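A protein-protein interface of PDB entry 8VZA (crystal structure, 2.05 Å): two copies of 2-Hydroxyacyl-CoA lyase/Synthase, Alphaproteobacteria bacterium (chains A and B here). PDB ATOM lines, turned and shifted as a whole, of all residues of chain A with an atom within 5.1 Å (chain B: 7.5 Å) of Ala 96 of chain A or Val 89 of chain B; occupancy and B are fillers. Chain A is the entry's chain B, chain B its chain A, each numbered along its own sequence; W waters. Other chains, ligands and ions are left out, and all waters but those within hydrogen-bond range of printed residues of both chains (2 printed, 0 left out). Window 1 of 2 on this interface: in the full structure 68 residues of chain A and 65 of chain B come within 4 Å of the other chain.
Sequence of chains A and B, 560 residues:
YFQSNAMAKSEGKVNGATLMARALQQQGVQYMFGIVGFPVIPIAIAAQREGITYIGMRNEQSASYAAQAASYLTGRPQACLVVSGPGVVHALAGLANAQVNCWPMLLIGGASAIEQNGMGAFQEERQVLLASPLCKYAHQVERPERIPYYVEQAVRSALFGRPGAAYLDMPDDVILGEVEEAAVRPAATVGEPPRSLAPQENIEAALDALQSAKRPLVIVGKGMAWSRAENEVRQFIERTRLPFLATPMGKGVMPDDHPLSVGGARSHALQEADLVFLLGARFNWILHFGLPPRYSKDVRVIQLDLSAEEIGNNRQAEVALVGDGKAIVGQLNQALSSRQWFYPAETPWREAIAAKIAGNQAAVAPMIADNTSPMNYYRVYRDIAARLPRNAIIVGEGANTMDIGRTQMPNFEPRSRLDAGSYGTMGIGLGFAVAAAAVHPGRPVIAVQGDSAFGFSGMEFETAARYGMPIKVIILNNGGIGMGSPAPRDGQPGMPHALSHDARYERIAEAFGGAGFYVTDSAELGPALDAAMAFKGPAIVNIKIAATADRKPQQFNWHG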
ATOM      1  N   VAL A  89      -1.960 -15.622 -14.676  1.00  0.00           N
ATOM      2  CA  VAL A  89      -1.129 -15.176 -15.798  1.00  0.00           C
ATOM      3  C   VAL A  89      -0.840 -13.678 -15.699  1.00  0.00           C
ATOM      4  O   VAL A  89       0.262 -13.225 -16.037  1.00  0.00           O
ATOM      5  CB  VAL A  89      -1.791 -15.538 -17.147  1.00  0.00           C
ATOM      6  CG1 VAL A  89      -0.854 -15.208 -18.314  1.00  0.00           C
ATOM      7  CG2 VAL A  89      -2.186 -17.022 -17.194  1.00  0.00           C
ATOM      8  N   LEU A  92       2.081 -13.331 -13.265  1.00  0.00           N
ATOM      9  CA  LEU A  92       3.417 -13.794 -13.633  1.00  0.00           C
ATOM     10  C   LEU A  92       4.420 -12.654 -13.714  1.00  0.00           C
ATOM     11  O   LEU A  92       5.627 -12.890 -13.584  1.00  0.00           O
ATOM     12  CB  LEU A  92       3.385 -14.528 -14.974  1.00  0.00           C
ATOM     13  CG  LEU A  92       2.521 -15.786 -15.060  1.00  0.00           C
ATOM     14  CD1 LEU A  92       2.590 -16.361 -16.466  1.00  0.00           C
ATOM     15  CD2 LEU A  92       2.949 -16.822 -14.029  1.00  0.00           C
ATOM     16  N   ALA A  93       3.946 -11.426 -13.931  1.00  0.00           N
ATOM     17  CA  ALA A  93       4.847 -10.285 -14.008  1.00  0.00           C
ATOM     18  C   ALA A  93       5.623 -10.120 -12.711  1.00  0.00           C
ATOM     19  O   ALA A  93       6.848  -9.942 -12.722  1.00  0.00           O
ATOM     20  CB  ALA A  93       4.051  -9.023 -14.326  1.00  0.00           C
ATOM     21  N   GLY A  94       4.920 -10.204 -11.581  1.00  0.00           N
ATOM     22  CA  GLY A  94       5.564 -10.002 -10.298  1.00  0.00           C
ATOM     23  C   GLY A  94       6.502 -11.133  -9.931  1.00  0.00           C
ATOM     24  O   GLY A  94       7.583 -10.896  -9.390  1.00  0.00           O
ATOM     25  N   LEU A  95       6.109 -12.375 -10.230  1.00  0.00           N
ATOM     26  CA  LEU A  95       7.000 -13.505  -9.981  1.00  0.00           C
ATOM     27  C   LEU A  95       8.328 -13.320 -10.704  1.00  0.00           C
ATOM     28  O   LEU A  95       9.398 -13.509 -10.114  1.00  0.00           O
ATOM     29  CB  LEU A  95       6.340 -14.815 -10.411  1.00  0.00           C
ATOM     30  CG  LEU A  95       5.014 -15.220  -9.766  1.00  0.00           C
ATOM     31  CD1 LEU A  95       4.584 -16.559 -10.321  1.00  0.00           C
ATOM     32  CD2 LEU A  95       5.116 -15.279  -8.250  1.00  0.00           C
ATOM     33  N   ALA A  96       8.276 -12.941 -11.986  1.00  0.00           N
ATOM     34  CA  ALA A  96       9.506 -12.736 -12.746  1.00  0.00           C
ATOM     35  C   ALA A  96      10.354 -11.625 -12.139  1.00  0.00           C
ATOM     36  O   ALA A  96      11.577 -11.762 -12.031  1.00  0.00           O
ATOM     37  CB  ALA A  96       9.178 -12.421 -14.208  1.00  0.00           C
ATOM     38  N   ASN A  97       9.725 -10.509 -11.752  1.00  0.00           N
ATOM     39  CA  ASN A  97      10.467  -9.408 -11.142  1.00  0.00           C
ATOM     40  C   ASN A  97      11.076  -9.825  -9.810  1.00  0.00           C
ATOM     41  O   ASN A  97      12.211  -9.451  -9.500  1.00  0.00           O
ATOM     42  CB  ASN A  97       9.556  -8.193 -10.954  1.00  0.00           C
ATOM     43  CG  ASN A  97      10.326  -6.908 -10.741  1.00  0.00           C
ATOM     44  OD1 ASN A  97      10.865  -6.338 -11.686  1.00  0.00           O
ATOM     45  ND2 ASN A  97      10.366  -6.429  -9.500  1.00  0.00           N
ATOM     46  N   ALA A  98      10.333 -10.590  -9.005  1.00  0.00           N
ATOM     47  CA  ALA A  98      10.866 -11.038  -7.722  1.00  0.00           C
ATOM     48  C   ALA A  98      12.053 -11.969  -7.916  1.00  0.00           C
ATOM     49  O   ALA A  98      13.024 -11.911  -7.153  1.00  0.00           O
ATOM     50  CB  ALA A  98       9.774 -11.724  -6.904  1.00  0.00           C
ATOM     51  N   GLN A  99      11.996 -12.825  -8.943  1.00  0.00           N
ATOM     52  CA  GLN A  99      13.098 -13.744  -9.219  1.00  0.00           C
ATOM     53  C   GLN A  99      14.370 -12.992  -9.597  1.00  0.00           C
ATOM     54  O   GLN A  99      15.471 -13.377  -9.193  1.00  0.00           O
ATOM     55  CB  GLN A  99      12.700 -14.712 -10.336  1.00  0.00           C
ATOM     56  CG  GLN A  99      13.764 -15.753 -10.712  1.00  0.00           C
ATOM     57  CD  GLN A  99      13.320 -16.644 -11.873  1.00  0.00           C
ATOM     58  OE1 GLN A  99      13.066 -16.162 -12.975  1.00  0.00           O
ATOM     59  NE2 GLN A  99      13.211 -17.946 -11.622  1.00  0.00           N
ATOM     60  N   VAL A 100      14.237 -11.921 -10.382  1.00  0.00           N
ATOM     61  CA  VAL A 100      15.413 -11.213 -10.878  1.00  0.00           C
ATOM     62  C   VAL A 100      16.049 -10.388  -9.767  1.00  0.00           C
ATOM     63  O   VAL A 100      17.278 -10.255  -9.699  1.00  0.00           O
ATOM     64  CB  VAL A 100      15.031 -10.346 -12.092  1.00  0.00           C
ATOM     65  CG1 VAL A 100      16.220  -9.521 -12.568  1.00  0.00           C
ATOM     66  CG2 VAL A 100      14.512 -11.225 -13.222  1.00  0.00           C
ATOM     67  N   LEU A 134       9.443 -19.333 -13.145  1.00  0.00           N
ATOM     68  CA  LEU A 134       9.652 -18.038 -12.514  1.00  0.00           C
ATOM     69  C   LEU A 134       9.738 -18.127 -10.995  1.00  0.00           C
ATOM     70  O   LEU A 134       9.850 -17.089 -10.330  1.00  0.00           O
ATOM     71  CB  LEU A 134       8.540 -17.071 -12.920  1.00  0.00           C
ATOM     72  CG  LEU A 134       8.492 -16.693 -14.399  1.00  0.00           C
ATOM     73  CD1 LEU A 134       7.301 -15.779 -14.683  1.00  0.00           C
ATOM     74  CD2 LEU A 134       9.802 -16.039 -14.833  1.00  0.00           C
ATOM     75  N   TYR A 423      15.375  -5.774 -13.149  1.00  0.00           N
ATOM     76  CA  TYR A 423      14.655  -6.183 -14.348  1.00  0.00           C
ATOM     77  C   TYR A 423      14.305  -5.007 -15.252  1.00  0.00           C
ATOM     78  O   TYR A 423      13.821  -5.228 -16.369  1.00  0.00           O
ATOM     79  CB  TYR A 423      13.363  -6.919 -13.959  1.00  0.00           C
ATOM     80  CG  TYR A 423      12.913  -8.005 -14.903  1.00  0.00           C
ATOM     81  CD1 TYR A 423      13.819  -8.675 -15.714  1.00  0.00           C
ATOM     82  CD2 TYR A 423      11.571  -8.370 -14.974  1.00  0.00           C
ATOM     83  CE1 TYR A 423      13.404  -9.672 -16.573  1.00  0.00           C
ATOM     84  CE2 TYR A 423      11.146  -9.364 -15.825  1.00  0.00           C
ATOM     85  CZ  TYR A 423      12.062 -10.011 -16.622  1.00  0.00           C
ATOM     86  OH  TYR A 423      11.631 -11.003 -17.470  1.00  0.00           O
ATOM     87  N   GLU B  60       1.389  -3.306 -21.575  1.00  0.00           N
ATOM     88  CA  GLU B  60       1.479  -4.416 -22.522  1.00  0.00           C
ATOM     89  C   GLU B  60       0.301  -5.369 -22.400  1.00  0.00           C
ATOM     90  O   GLU B  60      -0.011  -6.086 -23.356  1.00  0.00           O
ATOM     91  CB  GLU B  60       2.773  -5.203 -22.323  1.00  0.00           C
ATOM     92  CG  GLU B  60       4.022  -4.497 -22.789  1.00  0.00           C
ATOM     93  CD  GLU B  60       4.559  -3.557 -21.747  1.00  0.00           C
ATOM     94  OE1 GLU B  60       4.145  -3.672 -20.572  1.00  0.00           O
ATOM     95  OE2 GLU B  60       5.388  -2.701 -22.109  1.00  0.00           O
ATOM     96  N   GLN B  61      -0.324  -5.436 -21.221  1.00  0.00           N
ATOM     97  CA  GLN B  61      -1.512  -6.265 -21.044  1.00  0.00           C
ATOM     98  C   GLN B  61      -2.558  -5.925 -22.095  1.00  0.00           C
ATOM     99  O   GLN B  61      -2.962  -6.773 -22.899  1.00  0.00           O
ATOM    100  CB  GLN B  61      -2.077  -6.057 -19.637  1.00  0.00           C
ATOM    101  CG  GLN B  61      -2.386  -7.321 -18.876  1.00  0.00           C
ATOM    102  CD  GLN B  61      -2.948  -7.033 -17.495  1.00  0.00           C
ATOM    103  OE1 GLN B  61      -3.906  -6.272 -17.350  1.00  0.00           O
ATOM    104  NE2 GLN B  61      -2.345  -7.632 -16.469  1.00  0.00           N
ATOM    105  N   VAL B  82       6.577  -5.660 -27.917  1.00  0.00           N
ATOM    106  CA  VAL B  82       6.927  -5.413 -26.524  1.00  0.00           C
ATOM    107  C   VAL B  82       8.440  -5.478 -26.341  1.00  0.00           C
ATOM    108  O   VAL B  82       9.160  -6.124 -27.105  1.00  0.00           O
ATOM    109  CB  VAL B  82       6.228  -6.407 -25.563  1.00  0.00           C
ATOM    110  CG1 VAL B  82       4.717  -6.338 -25.732  1.00  0.00           C
ATOM    111  CG2 VAL B  82       6.734  -7.827 -25.786  1.00  0.00           C
ATOM    112  N   VAL B  83       8.914  -4.792 -25.300  1.00  0.00           N
ATOM    113  CA  VAL B  83      10.331  -4.778 -24.956  1.00  0.00           C
ATOM    114  C   VAL B  83      10.710  -6.122 -24.348  1.00  0.00           C
ATOM    115  O   VAL B  83       9.842  -6.942 -24.030  1.00  0.00           O
ATOM    116  CB  VAL B  83      10.667  -3.627 -23.989  1.00  0.00           C
ATOM    117  CG1 VAL B  83      10.168  -2.294 -24.535  1.00  0.00           C
ATOM    118  CG2 VAL B  83      10.087  -3.907 -22.595  1.00  0.00           C
ATOM    119  N   SER B  84      12.005  -6.346 -24.159  1.00  0.00           N
ATOM    120  CA  SER B  84      12.483  -7.568 -23.527  1.00  0.00           C
ATOM    121  C   SER B  84      12.055  -7.630 -22.057  1.00  0.00           C
ATOM    122  O   SER B  84      11.545  -6.664 -21.481  1.00  0.00           O
ATOM    123  CB  SER B  84      14.003  -7.649 -23.635  1.00  0.00           C
ATOM    124  OG  SER B  84      14.565  -6.351 -23.585  1.00  0.00           O
ATOM    125  N   GLY B  85      12.272  -8.797 -21.451  1.00  0.00           N
ATOM    126  CA  GLY B  85      12.029  -8.989 -20.040  1.00  0.00           C
ATOM    127  C   GLY B  85      10.579  -8.800 -19.656  1.00  0.00           C
ATOM    128  O   GLY B  85       9.690  -9.516 -20.127  1.00  0.00           O
ATOM    129  N   PRO B  86      10.307  -7.805 -18.807  1.00  0.00           N
ATOM    130  CA  PRO B  86       8.934  -7.633 -18.307  1.00  0.00           C
ATOM    131  C   PRO B  86       7.930  -7.274 -19.390  1.00  0.00           C
ATOM    132  O   PRO B  86       6.743  -7.593 -19.242  1.00  0.00           O
ATOM    133  CB  PRO B  86       9.086  -6.509 -17.273  1.00  0.00           C
ATOM    134  CG  PRO B  86      10.225  -5.709 -17.788  1.00  0.00           C
ATOM    135  CD  PRO B  86      11.196  -6.725 -18.347  1.00  0.00           C
ATOM    136  N   GLY B  87       8.354  -6.617 -20.472  1.00  0.00           N
ATOM    137  CA  GLY B  87       7.436  -6.406 -21.583  1.00  0.00           C
ATOM    138  C   GLY B  87       6.830  -7.710 -22.063  1.00  0.00           C
ATOM    139  O   GLY B  87       5.607  -7.848 -22.169  1.00  0.00           O
ATOM    140  N   VAL B  88       7.685  -8.700 -22.315  1.00  0.00           N
ATOM    141  CA  VAL B  88       7.215 -10.023 -22.707  1.00  0.00           C
ATOM    142  C   VAL B  88       6.384 -10.649 -21.595  1.00  0.00           C
ATOM    143  O   VAL B  88       5.324 -11.230 -21.851  1.00  0.00           O
ATOM    144  CB  VAL B  88       8.408 -10.917 -23.097  1.00  0.00           C
ATOM    145  CG1 VAL B  88       7.976 -12.369 -23.190  1.00  0.00           C
ATOM    146  CG2 VAL B  88       9.016 -10.444 -24.416  1.00  0.00           C
ATOM    147  N   VAL B  89       6.840 -10.536 -20.343  1.00  0.00           N
ATOM    148  CA  VAL B  89       6.115 -11.192 -19.258  1.00  0.00           C
ATOM    149  C   VAL B  89       4.744 -10.551 -19.064  1.00  0.00           C
ATOM    150  O   VAL B  89       3.757 -11.241 -18.787  1.00  0.00           O
ATOM    151  CB  VAL B  89       6.944 -11.183 -17.960  1.00  0.00           C
ATOM    152  CG1 VAL B  89       6.232 -11.990 -16.875  1.00  0.00           C
ATOM    153  CG2 VAL B  89       8.343 -11.752 -18.209  1.00  0.00           C
ATOM    154  N   HIS B  90       4.652  -9.228 -19.218  1.00  0.00           N
ATOM    155  CA  HIS B  90       3.344  -8.577 -19.176  1.00  0.00           C
ATOM    156  C   HIS B  90       2.435  -9.045 -20.313  1.00  0.00           C
ATOM    157  O   HIS B  90       1.213  -9.097 -20.145  1.00  0.00           O
ATOM    158  CB  HIS B  90       3.505  -7.054 -19.228  1.00  0.00           C
ATOM    159  CG  HIS B  90       4.017  -6.447 -17.955  1.00  0.00           C
ATOM    160  ND1 HIS B  90       3.948  -5.094 -17.695  1.00  0.00           N
ATOM    161  CD2 HIS B  90       4.614  -7.005 -16.877  1.00  0.00           C
ATOM    162  CE1 HIS B  90       4.472  -4.847 -16.508  1.00  0.00           C
ATOM    163  NE2 HIS B  90       4.884  -5.990 -15.991  1.00  0.00           N
ATOM    164  N   ALA B  91       3.000  -9.389 -21.472  1.00  0.00           N
ATOM    165  CA  ALA B  91       2.180  -9.785 -22.613  1.00  0.00           C
ATOM    166  C   ALA B  91       1.741 -11.247 -22.582  1.00  0.00           C
ATOM    167  O   ALA B  91       0.950 -11.649 -23.443  1.00  0.00           O
ATOM    168  CB  ALA B  91       2.921  -9.503 -23.922  1.00  0.00           C
ATOM    169  N   LEU B  92       2.209 -12.046 -21.613  1.00  0.00           N
ATOM    170  CA  LEU B  92       1.762 -13.436 -21.531  1.00  0.00           C
ATOM    171  C   LEU B  92       0.256 -13.535 -21.325  1.00  0.00           C
ATOM    172  O   LEU B  92      -0.358 -14.537 -21.712  1.00  0.00           O
ATOM    173  CB  LEU B  92       2.490 -14.168 -20.406  1.00  0.00           C
ATOM    174  CG  LEU B  92       4.015 -14.227 -20.515  1.00  0.00           C
ATOM    175  CD1 LEU B  92       4.600 -15.002 -19.336  1.00  0.00           C
ATOM    176  CD2 LEU B  92       4.434 -14.843 -21.834  1.00  0.00           C
ATOM    177  N   ALA B  93      -0.353 -12.509 -20.725  1.00  0.00           N
ATOM    178  CA  ALA B  93      -1.802 -12.506 -20.526  1.00  0.00           C
ATOM    179  C   ALA B  93      -2.545 -12.665 -21.850  1.00  0.00           C
ATOM    180  O   ALA B  93      -3.479 -13.470 -21.961  1.00  0.00           O
ATOM    181  CB  ALA B  93      -2.225 -11.217 -19.820  1.00  0.00           C
ATOM    182  N   GLY B  94      -2.131 -11.914 -22.872  1.00  0.00           N
ATOM    183  CA  GLY B  94      -2.799 -11.999 -24.161  1.00  0.00           C
ATOM    184  C   GLY B  94      -2.593 -13.331 -24.859  1.00  0.00           C
ATOM    185  O   GLY B  94      -3.517 -13.861 -25.489  1.00  0.00           O
ATOM    186  N   LEU B 107       2.905 -12.150 -31.337  1.00  0.00           N
ATOM    187  CA  LEU B 107       3.663 -11.384 -30.358  1.00  0.00           C
ATOM    188  C   LEU B 107       5.115 -11.312 -30.810  1.00  0.00           C
ATOM    189  O   LEU B 107       5.754 -12.350 -31.025  1.00  0.00           O
ATOM    190  CB  LEU B 107       3.560 -12.027 -28.974  1.00  0.00           C
ATOM    191  CG  LEU B 107       4.363 -11.348 -27.865  1.00  0.00           C
ATOM    192  CD1 LEU B 107       3.928  -9.895 -27.702  1.00  0.00           C
ATOM    193  CD2 LEU B 107       4.207 -12.109 -26.564  1.00  0.00           C
ATOM    194  N   GLU B 125      16.289 -12.739 -20.304  1.00  0.00           N
ATOM    195  CA  GLU B 125      15.196 -13.598 -19.863  1.00  0.00           C
ATOM    196  C   GLU B 125      15.038 -14.770 -20.825  1.00  0.00           C
ATOM    197  O   GLU B 125      15.328 -14.652 -22.017  1.00  0.00           O
ATOM    198  CB  GLU B 125      13.881 -12.816 -19.765  1.00  0.00           C
ATOM    199  CG  GLU B 125      12.728 -13.621 -19.194  1.00  0.00           C
ATOM    200  CD  GLU B 125      13.064 -14.199 -17.830  1.00  0.00           C
ATOM    201  OE1 GLU B 125      12.911 -13.471 -16.825  1.00  0.00           O
ATOM    202  OE2 GLU B 125      13.504 -15.371 -17.769  1.00  0.00           O
ATOM    203  N   ARG B 126      14.557 -15.899 -20.291  1.00  0.00           N
ATOM    204  CA  ARG B 126      14.240 -17.090 -21.087  1.00  0.00           C
ATOM    205  C   ARG B 126      12.838 -16.943 -21.685  1.00  0.00           C
ATOM    206  O   ARG B 126      11.866 -17.582 -21.277  1.00  0.00           O
ATOM    207  CB  ARG B 126      14.359 -18.342 -20.229  1.00  0.00           C
ATOM    208  CG  ARG B 126      15.670 -18.426 -19.461  1.00  0.00           C
ATOM    209  CD  ARG B 126      15.692 -19.613 -18.512  1.00  0.00           C
ATOM    210  NE  ARG B 126      14.694 -19.472 -17.459  1.00  0.00           N
ATOM    211  CZ  ARG B 126      14.392 -20.417 -16.581  1.00  0.00           C
ATOM    212  NH1 ARG B 126      14.994 -21.600 -16.601  1.00  0.00           N
ATOM    213  NH2 ARG B 126      13.463 -20.173 -15.662  1.00  0.00           N
ATOM    214  N   GLN B 127      12.753 -16.082 -22.700  1.00  0.00           N
ATOM    215  CA  GLN B 127      11.462 -15.615 -23.181  1.00  0.00           C
ATOM    216  C   GLN B 127      10.738 -16.673 -24.010  1.00  0.00           C
ATOM    217  O   GLN B 127       9.516 -16.818 -23.895  1.00  0.00           O
ATOM    218  CB  GLN B 127      11.660 -14.319 -23.970  1.00  0.00           C
ATOM    219  CG  GLN B 127      12.122 -13.176 -23.070  1.00  0.00           C
ATOM    220  CD  GLN B 127      12.620 -11.976 -23.842  1.00  0.00           C
ATOM    221  OE1 GLN B 127      13.337 -11.134 -23.300  1.00  0.00           O
ATOM    222  NE2 GLN B 127      12.253 -11.892 -25.115  1.00  0.00           N
ATOM    223  N   LEU B 130       9.272 -19.205 -21.537  1.00  0.00           N
ATOM    224  CA  LEU B 130       8.104 -18.753 -20.783  1.00  0.00           C
ATOM    225  C   LEU B 130       6.846 -18.776 -21.641  1.00  0.00           C
ATOM    226  O   LEU B 130       5.776 -19.183 -21.171  1.00  0.00           O
ATOM    227  CB  LEU B 130       8.339 -17.347 -20.229  1.00  0.00           C
ATOM    228  CG  LEU B 130       9.357 -17.170 -19.099  1.00  0.00           C
ATOM    229  CD1 LEU B 130       9.433 -15.714 -18.672  1.00  0.00           C
ATOM    230  CD2 LEU B 130       9.004 -18.052 -17.915  1.00  0.00           C
HETATM  231  O   HOH W   1       1.644 -11.486 -17.130  1.00  0.00           O
HETATM  232  O   HOH W   2      13.533 -17.571 -15.564  1.00  0.00           O
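The side-chain hydroxyl (OH) of Tyr 423 of chain A sits at hydrogen-bond distance from the side-chain carboxylate (OE1) of Glu 125 of chain B, 2.9 Å away.
OE1 of Glu 60 of chain B lies within hydrogen-bond range of ND1 of His 90 of chain B (3.2 Å). N of Gly 85 of chain B lies within hydrogen-bond range of OE1 of Gln 127 of chain B, 3.2 Å away.
Among the printed residues, merely in contact across the chains: Tyr 423 of chain A with Gly 85 of chain B (3.3 Å), Ala 93 of chain A with His 90 of chain B (3.3 Å), Tyr 423 of chain A with Val 89 of chain B (3.5 Å), Leu 92 of chain A with Val 89 of chain B (3.5 Å), Tyr 423 of chain A with Pro 86 of chain B (3.5 Å), Val 89 of chain A with Leu 92 of chain B (3.5 Å), Ala 93 of chain A with Val 89 of chain B (3.6 Å), Val 89 of chain A with Ala 93 of chain B (3.6 Å), Leu 92 of chain A with Leu 92 of chain B (3.8 Å), Leu 134 of chain A with Leu 130 of chain B (3.8 Å) and Ala 96 of chain A with Val 89 of chain B (3.997 Å).
Printed residues of chain B within 4 Å of Ala 96 of chain A: Val 89 (3.997 Å). Printed residues of chain A within 4 Å of Val 89 of chain B: Leu 92, Ala 93, Ala 96 and Tyr 423. Of the printed residues of chain B, Leu 92 of chain A touches Val 89 (3.5 Å) and Leu 92 (3.8 Å). Of the printed residues of chain A, Pro 86 of chain B touches Tyr 423. Of the printed residues of chain A, Leu 92 of chain B touches Val 89 and Leu 92. Gln 61 of chain B touches none of the printed residues of chain A. The nearest printed residue of chain B that does not touch Ala 96 of chain A is Glu 125 of chain B (4.7 Å). The nearest printed residue of chain A that does not touch Val 89 of chain B is Leu 134 of chain A (4.5 Å).
Of the 20 printed residues of chain B, 8 touch a printed residue of chain A. Hydrophobic or aromatic side chains of chain B within 4 Å of the printed part of chain A: Pro 86, Val 89, His 90, Leu 92 and Leu 130. Along chain B the printed residues that touch a printed residue of chain A span positions 85 to 130. Hydrophobic or aromatic side chains of chain A that line the printed part of chain B: Val 89, Leu 92, Ala 93, Ala 96, Leu 134 and Tyr 423. Among the printed residues, 12 pairs touch across the chains. Among the printed residues, no Asp or Glu carboxylate lies within 4 Å of a Lys or Arg side-chain nitrogen of the other chain.
Val 89 of chain A touches Leu 92 of chain B, and with the chains exchanged Leu 92 of chain A touches Val 89 of chain B. Val 89 of chain A touches Ala 93 of chain B, and with the chains exchanged Ala 93 of chain A touches Val 89 of chain B. Leu 92 of chain B touches its own counterpart, Leu 92 of chain A. Positions printed for both chains: 89, 92, 93 and 94.
Water W1 bridges O of Val 89 of chain A (2.5 Å) and O of Val 89 of chain B (2.7 Å). Water W2 lies within hydrogen-bond range of the guanidinium group (NH2) of Arg 126 of chain B (2.6 Å), the side-chain amide oxygen (OE1) of Gln 99 of chain A (3.0 Å) and the side-chain carboxylate (OE2) of Glu 125 of chain B (3.1 Å).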
